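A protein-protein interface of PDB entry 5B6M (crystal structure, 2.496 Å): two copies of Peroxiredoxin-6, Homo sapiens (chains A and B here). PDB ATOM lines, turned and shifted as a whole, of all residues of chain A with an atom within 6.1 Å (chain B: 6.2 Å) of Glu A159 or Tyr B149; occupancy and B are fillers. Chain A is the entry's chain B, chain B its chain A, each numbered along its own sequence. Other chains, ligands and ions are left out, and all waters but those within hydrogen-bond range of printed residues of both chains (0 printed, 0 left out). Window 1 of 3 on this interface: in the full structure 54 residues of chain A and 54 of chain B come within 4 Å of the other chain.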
ATOM      1  N   LEU A   7      12.696  -7.814  17.914  1.00  0.00           N
ATOM      2  CA  LEU A   7      12.033  -9.114  17.905  1.00  0.00           C
ATOM      3  C   LEU A   7      11.488  -9.391  16.512  1.00  0.00           C
ATOM      4  O   LEU A   7      10.961  -8.495  15.838  1.00  0.00           O
ATOM      5  CB  LEU A   7      10.892  -9.153  18.917  1.00  0.00           C
ATOM      6  CG  LEU A   7      11.280  -9.471  20.362  1.00  0.00           C
ATOM      7  CD1 LEU A   7      10.058  -9.608  21.246  1.00  0.00           C
ATOM      8  CD2 LEU A   7      12.142 -10.714  20.422  1.00  0.00           C
ATOM      9  N   LYS A 144      13.779 -14.190  19.167  1.00  0.00           N
ATOM     10  CA  LYS A 144      12.636 -14.524  20.004  1.00  0.00           C
ATOM     11  C   LYS A 144      12.749 -13.799  21.330  1.00  0.00           C
ATOM     12  O   LYS A 144      11.745 -13.529  21.979  1.00  0.00           O
ATOM     13  CB  LYS A 144      12.564 -16.026  20.253  1.00  0.00           C
ATOM     14  CG  LYS A 144      12.682 -16.906  19.014  1.00  0.00           C
ATOM     15  CD  LYS A 144      11.635 -16.572  17.979  1.00  0.00           C
ATOM     16  CE  LYS A 144      11.319 -17.776  17.087  1.00  0.00           C
ATOM     17  NZ  LYS A 144      10.331 -17.419  16.010  1.00  0.00           N
ATOM     18  N   LEU A 145      13.977 -13.465  21.721  1.00  0.00           N
ATOM     19  CA  LEU A 145      14.237 -12.799  22.989  1.00  0.00           C
ATOM     20  C   LEU A 145      15.635 -12.256  22.955  1.00  0.00           C
ATOM     21  O   LEU A 145      16.513 -12.855  22.343  1.00  0.00           O
ATOM     22  CB  LEU A 145      14.158 -13.804  24.137  1.00  0.00           C
ATOM     23  CG  LEU A 145      14.167 -13.317  25.585  1.00  0.00           C
ATOM     24  CD1 LEU A 145      13.107 -14.079  26.387  1.00  0.00           C
ATOM     25  CD2 LEU A 145      15.530 -13.490  26.205  1.00  0.00           C
ATOM     26  N   SER A 146      15.859 -11.134  23.627  1.00  0.00           N
ATOM     27  CA  SER A 146      17.220 -10.650  23.817  1.00  0.00           C
ATOM     28  C   SER A 146      17.420  -9.885  25.138  1.00  0.00           C
ATOM     29  O   SER A 146      16.471  -9.373  25.739  1.00  0.00           O
ATOM     30  CB  SER A 146      17.633  -9.786  22.632  1.00  0.00           C
ATOM     31  OG  SER A 146      16.929  -8.575  22.701  1.00  0.00           O
ATOM     32  N   ILE A 147      18.656  -9.838  25.613  1.00  0.00           N
ATOM     33  CA  ILE A 147      18.963  -9.048  26.798  1.00  0.00           C
ATOM     34  C   ILE A 147      20.251  -8.268  26.604  1.00  0.00           C
ATOM     35  O   ILE A 147      21.135  -8.686  25.865  1.00  0.00           O
ATOM     36  CB  ILE A 147      19.009  -9.894  28.099  1.00  0.00           C
ATOM     37  CG1 ILE A 147      20.445 -10.114  28.581  1.00  0.00           C
ATOM     38  CG2 ILE A 147      18.262 -11.229  27.946  1.00  0.00           C
ATOM     39  CD1 ILE A 147      20.534 -10.844  29.907  1.00  0.00           C
ATOM     40  N   TYR A 149      23.013  -6.549  28.938  1.00  0.00           N
ATOM     41  CA  TYR A 149      23.618  -6.199  30.220  1.00  0.00           C
ATOM     42  C   TYR A 149      24.939  -5.453  30.004  1.00  0.00           C
ATOM     43  O   TYR A 149      25.630  -5.682  29.013  1.00  0.00           O
ATOM     44  CB  TYR A 149      23.816  -7.425  31.124  1.00  0.00           C
ATOM     45  CG  TYR A 149      22.586  -7.952  31.820  1.00  0.00           C
ATOM     46  CD1 TYR A 149      21.319  -7.718  31.321  1.00  0.00           C
ATOM     47  CD2 TYR A 149      22.696  -8.697  32.994  1.00  0.00           C
ATOM     48  CE1 TYR A 149      20.185  -8.224  31.979  1.00  0.00           C
ATOM     49  CE2 TYR A 149      21.578  -9.198  33.654  1.00  0.00           C
ATOM     50  CZ  TYR A 149      20.329  -8.963  33.139  1.00  0.00           C
ATOM     51  OH  TYR A 149      19.221  -9.467  33.764  1.00  0.00           O
ATOM     52  N   ASN A 156      22.380 -13.572  34.587  1.00  0.00           N
ATOM     53  CA  ASN A 156      21.804 -14.643  35.361  1.00  0.00           C
ATOM     54  C   ASN A 156      21.446 -15.779  34.405  1.00  0.00           C
ATOM     55  O   ASN A 156      20.402 -15.764  33.746  1.00  0.00           O
ATOM     56  CB  ASN A 156      20.601 -14.107  36.137  1.00  0.00           C
ATOM     57  CG  ASN A 156      19.730 -15.204  36.760  1.00  0.00           C
ATOM     58  OD1 ASN A 156      19.948 -16.404  36.593  1.00  0.00           O
ATOM     59  ND2 ASN A 156      18.718 -14.768  37.493  1.00  0.00           N
ATOM     60  N   PHE A 157      22.318 -16.774  34.335  1.00  0.00           N
ATOM     61  CA  PHE A 157      22.143 -17.863  33.397  1.00  0.00           C
ATOM     62  C   PHE A 157      21.027 -18.825  33.723  1.00  0.00           C
ATOM     63  O   PHE A 157      20.590 -19.591  32.862  1.00  0.00           O
ATOM     64  CB  PHE A 157      23.440 -18.629  33.211  1.00  0.00           C
ATOM     65  CG  PHE A 157      24.229 -18.171  32.037  1.00  0.00           C
ATOM     66  CD1 PHE A 157      24.915 -16.972  32.079  1.00  0.00           C
ATOM     67  CD2 PHE A 157      24.282 -18.929  30.892  1.00  0.00           C
ATOM     68  CE1 PHE A 157      25.650 -16.531  30.999  1.00  0.00           C
ATOM     69  CE2 PHE A 157      25.017 -18.500  29.813  1.00  0.00           C
ATOM     70  CZ  PHE A 157      25.700 -17.290  29.869  1.00  0.00           C
ATOM     71  N   ASP A 158      20.538 -18.799  34.945  1.00  0.00           N
ATOM     72  CA  ASP A 158      19.402 -19.643  35.226  1.00  0.00           C
ATOM     73  C   ASP A 158      18.152 -19.014  34.632  1.00  0.00           C
ATOM     74  O   ASP A 158      17.203 -19.720  34.321  1.00  0.00           O
ATOM     75  CB  ASP A 158      19.276 -19.944  36.719  1.00  0.00           C
ATOM     76  CG  ASP A 158      20.467 -20.751  37.256  1.00  0.00           C
ATOM     77  OD1 ASP A 158      21.635 -20.438  36.893  1.00  0.00           O
ATOM     78  OD2 ASP A 158      20.245 -21.691  38.043  1.00  0.00           O
ATOM     79  N   GLU A 159      18.175 -17.694  34.447  1.00  0.00           N
ATOM     80  CA  GLU A 159      17.047 -16.993  33.853  1.00  0.00           C
ATOM     81  C   GLU A 159      17.028 -17.216  32.324  1.00  0.00           C
ATOM     82  O   GLU A 159      15.961 -17.439  31.734  1.00  0.00           O
ATOM     83  CB  GLU A 159      17.063 -15.505  34.225  1.00  0.00           C
ATOM     84  CG  GLU A 159      16.135 -14.622  33.386  1.00  0.00           C
ATOM     85  CD  GLU A 159      14.640 -14.783  33.692  1.00  0.00           C
ATOM     86  OE1 GLU A 159      14.265 -15.616  34.530  1.00  0.00           O
ATOM     87  OE2 GLU A 159      13.813 -14.059  33.091  1.00  0.00           O
ATOM     88  N   ILE A 160      18.208 -17.170  31.701  1.00  0.00           N
ATOM     89  CA  ILE A 160      18.348 -17.580  30.311  1.00  0.00           C
ATOM     90  C   ILE A 160      17.738 -18.955  30.077  1.00  0.00           C
ATOM     91  O   ILE A 160      16.931 -19.111  29.179  1.00  0.00           O
ATOM     92  CB  ILE A 160      19.823 -17.579  29.844  1.00  0.00           C
ATOM     93  CG1 ILE A 160      20.299 -16.152  29.577  1.00  0.00           C
ATOM     94  CG2 ILE A 160      19.993 -18.390  28.571  1.00  0.00           C
ATOM     95  CD1 ILE A 160      21.762 -15.986  29.761  1.00  0.00           C
ATOM     96  N   LEU A 161      18.085 -19.951  30.892  1.00  0.00           N
ATOM     97  CA  LEU A 161      17.533 -21.286  30.669  1.00  0.00           C
ATOM     98  C   LEU A 161      16.035 -21.272  30.842  1.00  0.00           C
ATOM     99  O   LEU A 161      15.305 -21.927  30.096  1.00  0.00           O
ATOM    100  CB  LEU A 161      18.136 -22.314  31.617  1.00  0.00           C
ATOM    101  CG  LEU A 161      17.569 -23.706  31.354  1.00  0.00           C
ATOM    102  CD1 LEU A 161      18.077 -24.261  30.036  1.00  0.00           C
ATOM    103  CD2 LEU A 161      17.888 -24.644  32.488  1.00  0.00           C
ATOM    104  N   ARG A 162      15.578 -20.503  31.820  1.00  0.00           N
ATOM    105  CA  ARG A 162      14.165 -20.434  32.156  1.00  0.00           C
ATOM    106  C   ARG A 162      13.384 -19.893  30.941  1.00  0.00           C
ATOM    107  O   ARG A 162      12.417 -20.517  30.500  1.00  0.00           O
ATOM    108  CB  ARG A 162      13.961 -19.549  33.395  1.00  0.00           C
ATOM    109  CG  ARG A 162      12.535 -19.479  33.885  1.00  0.00           C
ATOM    110  CD  ARG A 162      12.318 -18.336  34.874  1.00  0.00           C
ATOM    111  NE  ARG A 162      12.344 -17.017  34.255  1.00  0.00           N
ATOM    112  CZ  ARG A 162      11.263 -16.425  33.744  1.00  0.00           C
ATOM    113  NH1 ARG A 162      10.091 -17.043  33.809  1.00  0.00           N
ATOM    114  NH2 ARG A 162      11.347 -15.220  33.175  1.00  0.00           N
ATOM    115  N   VAL A 163      13.810 -18.749  30.395  1.00  0.00           N
ATOM    116  CA  VAL A 163      13.104 -18.180  29.239  1.00  0.00           C
ATOM    117  C   VAL A 163      13.206 -19.090  28.029  1.00  0.00           C
ATOM    118  O   VAL A 163      12.337 -19.108  27.201  1.00  0.00           O
ATOM    119  CB  VAL A 163      13.553 -16.743  28.839  1.00  0.00           C
ATOM    120  CG1 VAL A 163      13.328 -15.774  29.970  1.00  0.00           C
ATOM    121  CG2 VAL A 163      14.994 -16.714  28.381  1.00  0.00           C
ATOM    122  N   VAL A 164      14.274 -19.848  27.932  1.00  0.00           N
ATOM    123  CA  VAL A 164      14.380 -20.816  26.866  1.00  0.00           C
ATOM    124  C   VAL A 164      13.313 -21.885  27.023  1.00  0.00           C
ATOM    125  O   VAL A 164      12.727 -22.305  26.037  1.00  0.00           O
ATOM    126  CB  VAL A 164      15.779 -21.461  26.813  1.00  0.00           C
ATOM    127  CG1 VAL A 164      15.730 -22.795  26.081  1.00  0.00           C
ATOM    128  CG2 VAL A 164      16.752 -20.514  26.156  1.00  0.00           C
ATOM    129  N   ASP B 118       6.136  -6.179  19.451  1.00  0.00           N
ATOM    130  CA  ASP B 118       6.094  -7.634  19.412  1.00  0.00           C
ATOM    131  C   ASP B 118       5.783  -8.076  17.979  1.00  0.00           C
ATOM    132  O   ASP B 118       4.880  -7.543  17.327  1.00  0.00           O
ATOM    133  CB  ASP B 118       5.073  -8.184  20.420  1.00  0.00           C
ATOM    134  CG  ASP B 118       5.174  -9.704  20.611  1.00  0.00           C
ATOM    135  OD1 ASP B 118       5.810 -10.147  21.590  1.00  0.00           O
ATOM    136  OD2 ASP B 118       4.601 -10.457  19.789  1.00  0.00           O
ATOM    137  N   ALA B 131       6.119  -5.541  22.946  1.00  0.00           N
ATOM    138  CA  ALA B 131       6.484  -6.748  23.653  1.00  0.00           C
ATOM    139  C   ALA B 131       6.639  -6.481  25.165  1.00  0.00           C
ATOM    140  O   ALA B 131       6.098  -5.507  25.707  1.00  0.00           O
ATOM    141  CB  ALA B 131       7.741  -7.322  23.058  1.00  0.00           C
ATOM    142  N   ARG B 132       7.370  -7.362  25.845  1.00  0.00           N
ATOM    143  CA  ARG B 132       7.654  -7.170  27.273  1.00  0.00           C
ATOM    144  C   ARG B 132       9.051  -6.573  27.496  1.00  0.00           C
ATOM    145  O   ARG B 132       9.998  -7.280  27.827  1.00  0.00           O
ATOM    146  CB  ARG B 132       7.445  -8.462  28.059  1.00  0.00           C
ATOM    147  CG  ARG B 132       5.989  -8.809  28.203  1.00  0.00           C
ATOM    148  CD  ARG B 132       5.725 -10.231  28.698  1.00  0.00           C
ATOM    149  NE  ARG B 132       4.394 -10.658  28.280  1.00  0.00           N
ATOM    150  CZ  ARG B 132       3.258 -10.166  28.777  1.00  0.00           C
ATOM    151  NH1 ARG B 132       3.292  -9.241  29.733  1.00  0.00           N
ATOM    152  NH2 ARG B 132       2.086 -10.597  28.322  1.00  0.00           N
ATOM    153  N   VAL B 133       9.149  -5.259  27.318  1.00  0.00           N
ATOM    154  CA  VAL B 133      10.427  -4.565  27.278  1.00  0.00           C
ATOM    155  C   VAL B 133      10.718  -3.903  28.628  1.00  0.00           C
ATOM    156  O   VAL B 133       9.800  -3.453  29.299  1.00  0.00           O
ATOM    157  CB  VAL B 133      10.395  -3.500  26.137  1.00  0.00           C
ATOM    158  CG1 VAL B 133      11.683  -2.715  26.044  1.00  0.00           C
ATOM    159  CG2 VAL B 133      10.088  -4.178  24.815  1.00  0.00           C
ATOM    160  N   VAL B 134      11.987  -3.858  29.024  1.00  0.00           N
ATOM    161  CA  VAL B 134      12.416  -3.078  30.177  1.00  0.00           C
ATOM    162  C   VAL B 134      13.594  -2.175  29.769  1.00  0.00           C
ATOM    163  O   VAL B 134      14.520  -2.622  29.097  1.00  0.00           O
ATOM    164  CB  VAL B 134      12.847  -4.009  31.358  1.00  0.00           C
ATOM    165  CG1 VAL B 134      13.211  -3.207  32.579  1.00  0.00           C
ATOM    166  CG2 VAL B 134      11.772  -5.032  31.679  1.00  0.00           C
ATOM    167  N   ILE B 147      16.100  -5.208  28.440  1.00  0.00           N
ATOM    168  CA  ILE B 147      15.596  -6.562  28.323  1.00  0.00           C
ATOM    169  C   ILE B 147      14.452  -6.511  27.300  1.00  0.00           C
ATOM    170  O   ILE B 147      13.708  -5.525  27.235  1.00  0.00           O
ATOM    171  CB  ILE B 147      15.081  -7.045  29.706  1.00  0.00           C
ATOM    172  CG1 ILE B 147      16.228  -7.159  30.698  1.00  0.00           C
ATOM    173  CG2 ILE B 147      14.415  -8.365  29.619  1.00  0.00           C
ATOM    174  CD1 ILE B 147      15.742  -7.284  32.118  1.00  0.00           C
ATOM    175  N   LEU B 148      14.316  -7.557  26.496  1.00  0.00           N
ATOM    176  CA  LEU B 148      13.351  -7.544  25.410  1.00  0.00           C
ATOM    177  C   LEU B 148      12.781  -8.919  25.333  1.00  0.00           C
ATOM    178  O   LEU B 148      13.383  -9.819  24.752  1.00  0.00           O
ATOM    179  CB  LEU B 148      14.040  -7.201  24.090  1.00  0.00           C
ATOM    180  CG  LEU B 148      13.220  -6.418  23.052  1.00  0.00           C
ATOM    181  CD1 LEU B 148      14.015  -6.116  21.765  1.00  0.00           C
ATOM    182  CD2 LEU B 148      11.918  -7.129  22.722  1.00  0.00           C
ATOM    183  N   TYR B 149      11.616  -9.078  25.939  1.00  0.00           N
ATOM    184  CA  TYR B 149      10.948 -10.371  26.016  1.00  0.00           C
ATOM    185  C   TYR B 149       9.671 -10.361  25.173  1.00  0.00           C
ATOM    186  O   TYR B 149       9.005  -9.337  25.098  1.00  0.00           O
ATOM    187  CB  TYR B 149      10.573 -10.679  27.460  1.00  0.00           C
ATOM    188  CG  TYR B 149      11.664 -11.235  28.352  1.00  0.00           C
ATOM    189  CD1 TYR B 149      13.005 -10.978  28.119  1.00  0.00           C
ATOM    190  CD2 TYR B 149      11.332 -12.036  29.453  1.00  0.00           C
ATOM    191  CE1 TYR B 149      13.982 -11.504  28.956  1.00  0.00           C
ATOM    192  CE2 TYR B 149      12.284 -12.547  30.280  1.00  0.00           C
ATOM    193  CZ  TYR B 149      13.609 -12.286  30.035  1.00  0.00           C
ATOM    194  OH  TYR B 149      14.548 -12.822  30.885  1.00  0.00           O
ATOM    195  N   PRO B 150       9.318 -11.511  24.567  1.00  0.00           N
ATOM    196  CA  PRO B 150       8.078 -11.686  23.809  1.00  0.00           C
ATOM    197  C   PRO B 150       6.840 -11.662  24.726  1.00  0.00           C
ATOM    198  O   PRO B 150       6.953 -11.774  25.958  1.00  0.00           O
ATOM    199  CB  PRO B 150       8.242 -13.088  23.217  1.00  0.00           C
ATOM    200  CG  PRO B 150       9.102 -13.804  24.181  1.00  0.00           C
ATOM    201  CD  PRO B 150      10.066 -12.778  24.671  1.00  0.00           C
ATOM    202  N   ALA B 151       5.661 -11.531  24.122  1.00  0.00           N
ATOM    203  CA  ALA B 151       4.413 -11.475  24.872  1.00  0.00           C
ATOM    204  C   ALA B 151       4.012 -12.827  25.492  1.00  0.00           C
ATOM    205  O   ALA B 151       3.295 -12.864  26.497  1.00  0.00           O
ATOM    206  CB  ALA B 151       3.312 -10.948  23.985  1.00  0.00           C
ATOM    207  N   THR B 153       6.066 -14.801  26.986  1.00  0.00           N
ATOM    208  CA  THR B 153       6.981 -15.120  28.091  1.00  0.00           C
ATOM    209  C   THR B 153       7.135 -13.998  29.124  1.00  0.00           C
ATOM    210  O   THR B 153       7.874 -13.036  28.911  1.00  0.00           O
ATOM    211  CB  THR B 153       8.385 -15.538  27.554  1.00  0.00           C
ATOM    212  OG1 THR B 153       8.272 -16.758  26.804  1.00  0.00           O
ATOM    213  CG2 THR B 153       9.344 -15.758  28.695  1.00  0.00           C
ATOM    214  N   GLY B 154       6.440 -14.129  30.248  1.00  0.00           N
ATOM    215  CA  GLY B 154       6.539 -13.155  31.331  1.00  0.00           C
ATOM    216  C   GLY B 154       7.936 -12.990  31.909  1.00  0.00           C
ATOM    217  O   GLY B 154       8.733 -13.932  31.905  1.00  0.00           O
ATOM    218  N   ARG B 155       8.224 -11.791  32.405  1.00  0.00           N
ATOM    219  CA  ARG B 155       9.553 -11.459  32.910  1.00  0.00           C
ATOM    220  C   ARG B 155       9.858 -11.987  34.328  1.00  0.00           C
ATOM    221  O   ARG B 155       8.999 -12.545  35.019  1.00  0.00           O
ATOM    222  CB  ARG B 155       9.765  -9.951  32.862  1.00  0.00           C
ATOM    223  CG  ARG B 155      10.016  -9.423  31.459  1.00  0.00           C
ATOM    224  CD  ARG B 155       9.691  -7.946  31.319  1.00  0.00           C
ATOM    225  NE  ARG B 155       8.252  -7.707  31.266  1.00  0.00           N
ATOM    226  CZ  ARG B 155       7.696  -6.545  30.929  1.00  0.00           C
ATOM    227  NH1 ARG B 155       8.474  -5.522  30.605  1.00  0.00           N
ATOM    228  NH2 ARG B 155       6.365  -6.407  30.915  1.00  0.00           N
ATOM    229  N   ASN B 156      11.093 -11.807  34.755  1.00  0.00           N
ATOM    230  CA  ASN B 156      11.451 -12.124  36.113  1.00  0.00           C
ATOM    231  C   ASN B 156      11.667 -10.793  36.814  1.00  0.00           C
ATOM    232  O   ASN B 156      12.625 -10.071  36.531  1.00  0.00           O
ATOM    233  CB  ASN B 156      12.711 -13.001  36.120  1.00  0.00           C
ATOM    234  CG  ASN B 156      13.252 -13.290  37.528  1.00  0.00           C
ATOM    235  OD1 ASN B 156      13.043 -12.528  38.480  1.00  0.00           O
ATOM    236  ND2 ASN B 156      13.997 -14.385  37.644  1.00  0.00           N
ATOM    237  N   GLU B 159      14.807 -10.636  39.190  1.00  0.00           N
ATOM    238  CA  GLU B 159      15.988 -10.364  38.384  1.00  0.00           C
ATOM    239  C   GLU B 159      16.108  -8.886  38.064  1.00  0.00           C
ATOM    240  O   GLU B 159      17.195  -8.310  38.137  1.00  0.00           O
ATOM    241  CB  GLU B 159      15.946 -11.188  37.092  1.00  0.00           C
ATOM    242  CG  GLU B 159      17.012 -10.846  36.097  1.00  0.00           C
ATOM    243  CD  GLU B 159      18.406 -11.141  36.607  1.00  0.00           C
ATOM    244  OE1 GLU B 159      18.552 -11.997  37.518  1.00  0.00           O
ATOM    245  OE2 GLU B 159      19.354 -10.525  36.075  1.00  0.00           O
ATOM    246  N   ASP B 180      25.097 -14.709  38.113  1.00  0.00           N
ATOM    247  CA  ASP B 180      24.162 -15.205  39.123  1.00  0.00           C
ATOM    248  C   ASP B 180      24.290 -14.550  40.481  1.00  0.00           C
ATOM    249  O   ASP B 180      23.646 -14.992  41.429  1.00  0.00           O
ATOM    250  CB  ASP B 180      24.269 -16.726  39.286  1.00  0.00           C
ATOM    251  CG  ASP B 180      24.041 -17.447  38.000  1.00  0.00           C
ATOM    252  OD1 ASP B 180      23.451 -16.819  37.099  1.00  0.00           O
ATOM    253  OD2 ASP B 180      24.447 -18.623  37.879  1.00  0.00           O
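Of chain B, only Tyr B149 (2.6 Å) and Asn B156 (3.4 Å) come within 4 Å of Glu A159. Of the printed residues of chain A, Tyr B149 touches Leu A145 (3.6 Å), Glu A159 (2.6 Å) and Val A163 (3.3 Å). Printed residues of chain B within 4 Å of Leu A145: Leu B148 (3.6 Å), Tyr B149 (3.6 Å) and Pro B150 (3.7 Å). Of the printed residues of chain A, Asn B156 touches Glu A159 and Arg A162. Printed residues of chain B within 4 Å of Phe A157: Asp B180 (3.0 Å). Printed residues of chain A within 4 Å of Pro B150: Leu A7 (3.8 Å), Lys A144 (3.3 Å) and Leu A145 (3.7 Å). Of the printed residues of chain A, Arg B155 touches Arg A162 (3.7 Å). The nearest residue of chain B that does not touch Glu A159 is Arg B155 (4.6 Å). The nearest printed residue of chain A that does not touch Tyr B149 is Leu A7 (4.003 Å). The nearest printed residue of chain A that does not touch Asp B180 is Glu A159 (6.0 Å).
OD1 of Asn A156 lies within hydrogen-bond range of N of Glu A159, at 3.1 Å. The backbone NH of Val B134 sits at hydrogen-bond distance from the backbone carbonyl oxygen of Ile B147, 3.0 Å away. The backbone carbonyl oxygen of Val B133 sits at hydrogen-bond distance from the guanidinium group of Arg B155. OD1 of Asn A156 is in hydrogen-bond range of N of Asp A158 (3.0 Å). The backbone carbonyl oxygen (O) of Tyr B149 is in hydrogen-bond range of the backbone NH (N) of Arg B132, at 2.7 Å. OE2 of Glu A159 is in salt-bridge range of NH2 of Arg A162 (2.7 Å).
Of the 16 printed residues of chain B, 10 touch a printed residue of chain A. Printed residues of chain B that touch a printed residue of chain A: Ala B131, Ile B147, Leu B148, Tyr B149, Pro B150, Gly B154, Arg B155, Asn B156, Glu B159 and Asp B180.
Tyr A149 touches Glu B159, and with the chains exchanged Glu A159 touches Tyr B149. Asn A156 touches Glu B159, and with the chains exchanged Glu A159 touches Asn B156. Of the 20 pairs that touch across the chains among the printed residues, 4 have their exchanged pair printed and touching as well.
Leu A7 touches Ala B131 (CD1 to CB, 3.7 Å). CD2 of Leu B148 touches CG of Leu A7, at 3.4 Å. Leu A7 touches Pro B150. O of Lys A144 touches CD of Pro B150 (3.3 Å). Leu A145 touches Leu B148 (CA to O, 3.6 Å). Leu A145 touches Pro B150. Ser A146 touches Ile B147 (O to C, 3.8 Å). Asn A156 touches Asp B180 (CA to OD1, 3.2 Å). NH2 of Arg A162 touches C of Arg B155 (3.7 Å). Tyr B149 touches Val A163.
The side-chain amide nitrogen (ND2) of Asn B156 is in hydrogen-bond range of the side-chain carboxylate (OE1) of Glu A159 (3.4 Å). The backbone carbonyl oxygen (O) of Gly B154 lies within hydrogen-bond range of the guanidinium group (NH2) of Arg A162 (3.2 Å). The side-chain carboxylate of Glu B159 lies within hydrogen-bond range of the side-chain amide nitrogen of Asn A156. O of Ser A146 is in hydrogen-bond range of N of Leu B148 (2.9 Å). OD1 of Asp B180 sits at hydrogen-bond distance from N of Phe A157, at 3.0 Å. The side-chain carboxylate (OD1) of Asp A158 lies close to the side-chain carboxylate (OD2) of Asp B180, at 3.5 Å. OH of Tyr A149 sits at hydrogen-bond distance from OE2 of Glu B159, 2.5 Å away. The side-chain hydroxyl of Tyr B149 is in hydrogen-bond range of the side-chain carboxylate of Glu A159 (2.6 Å).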
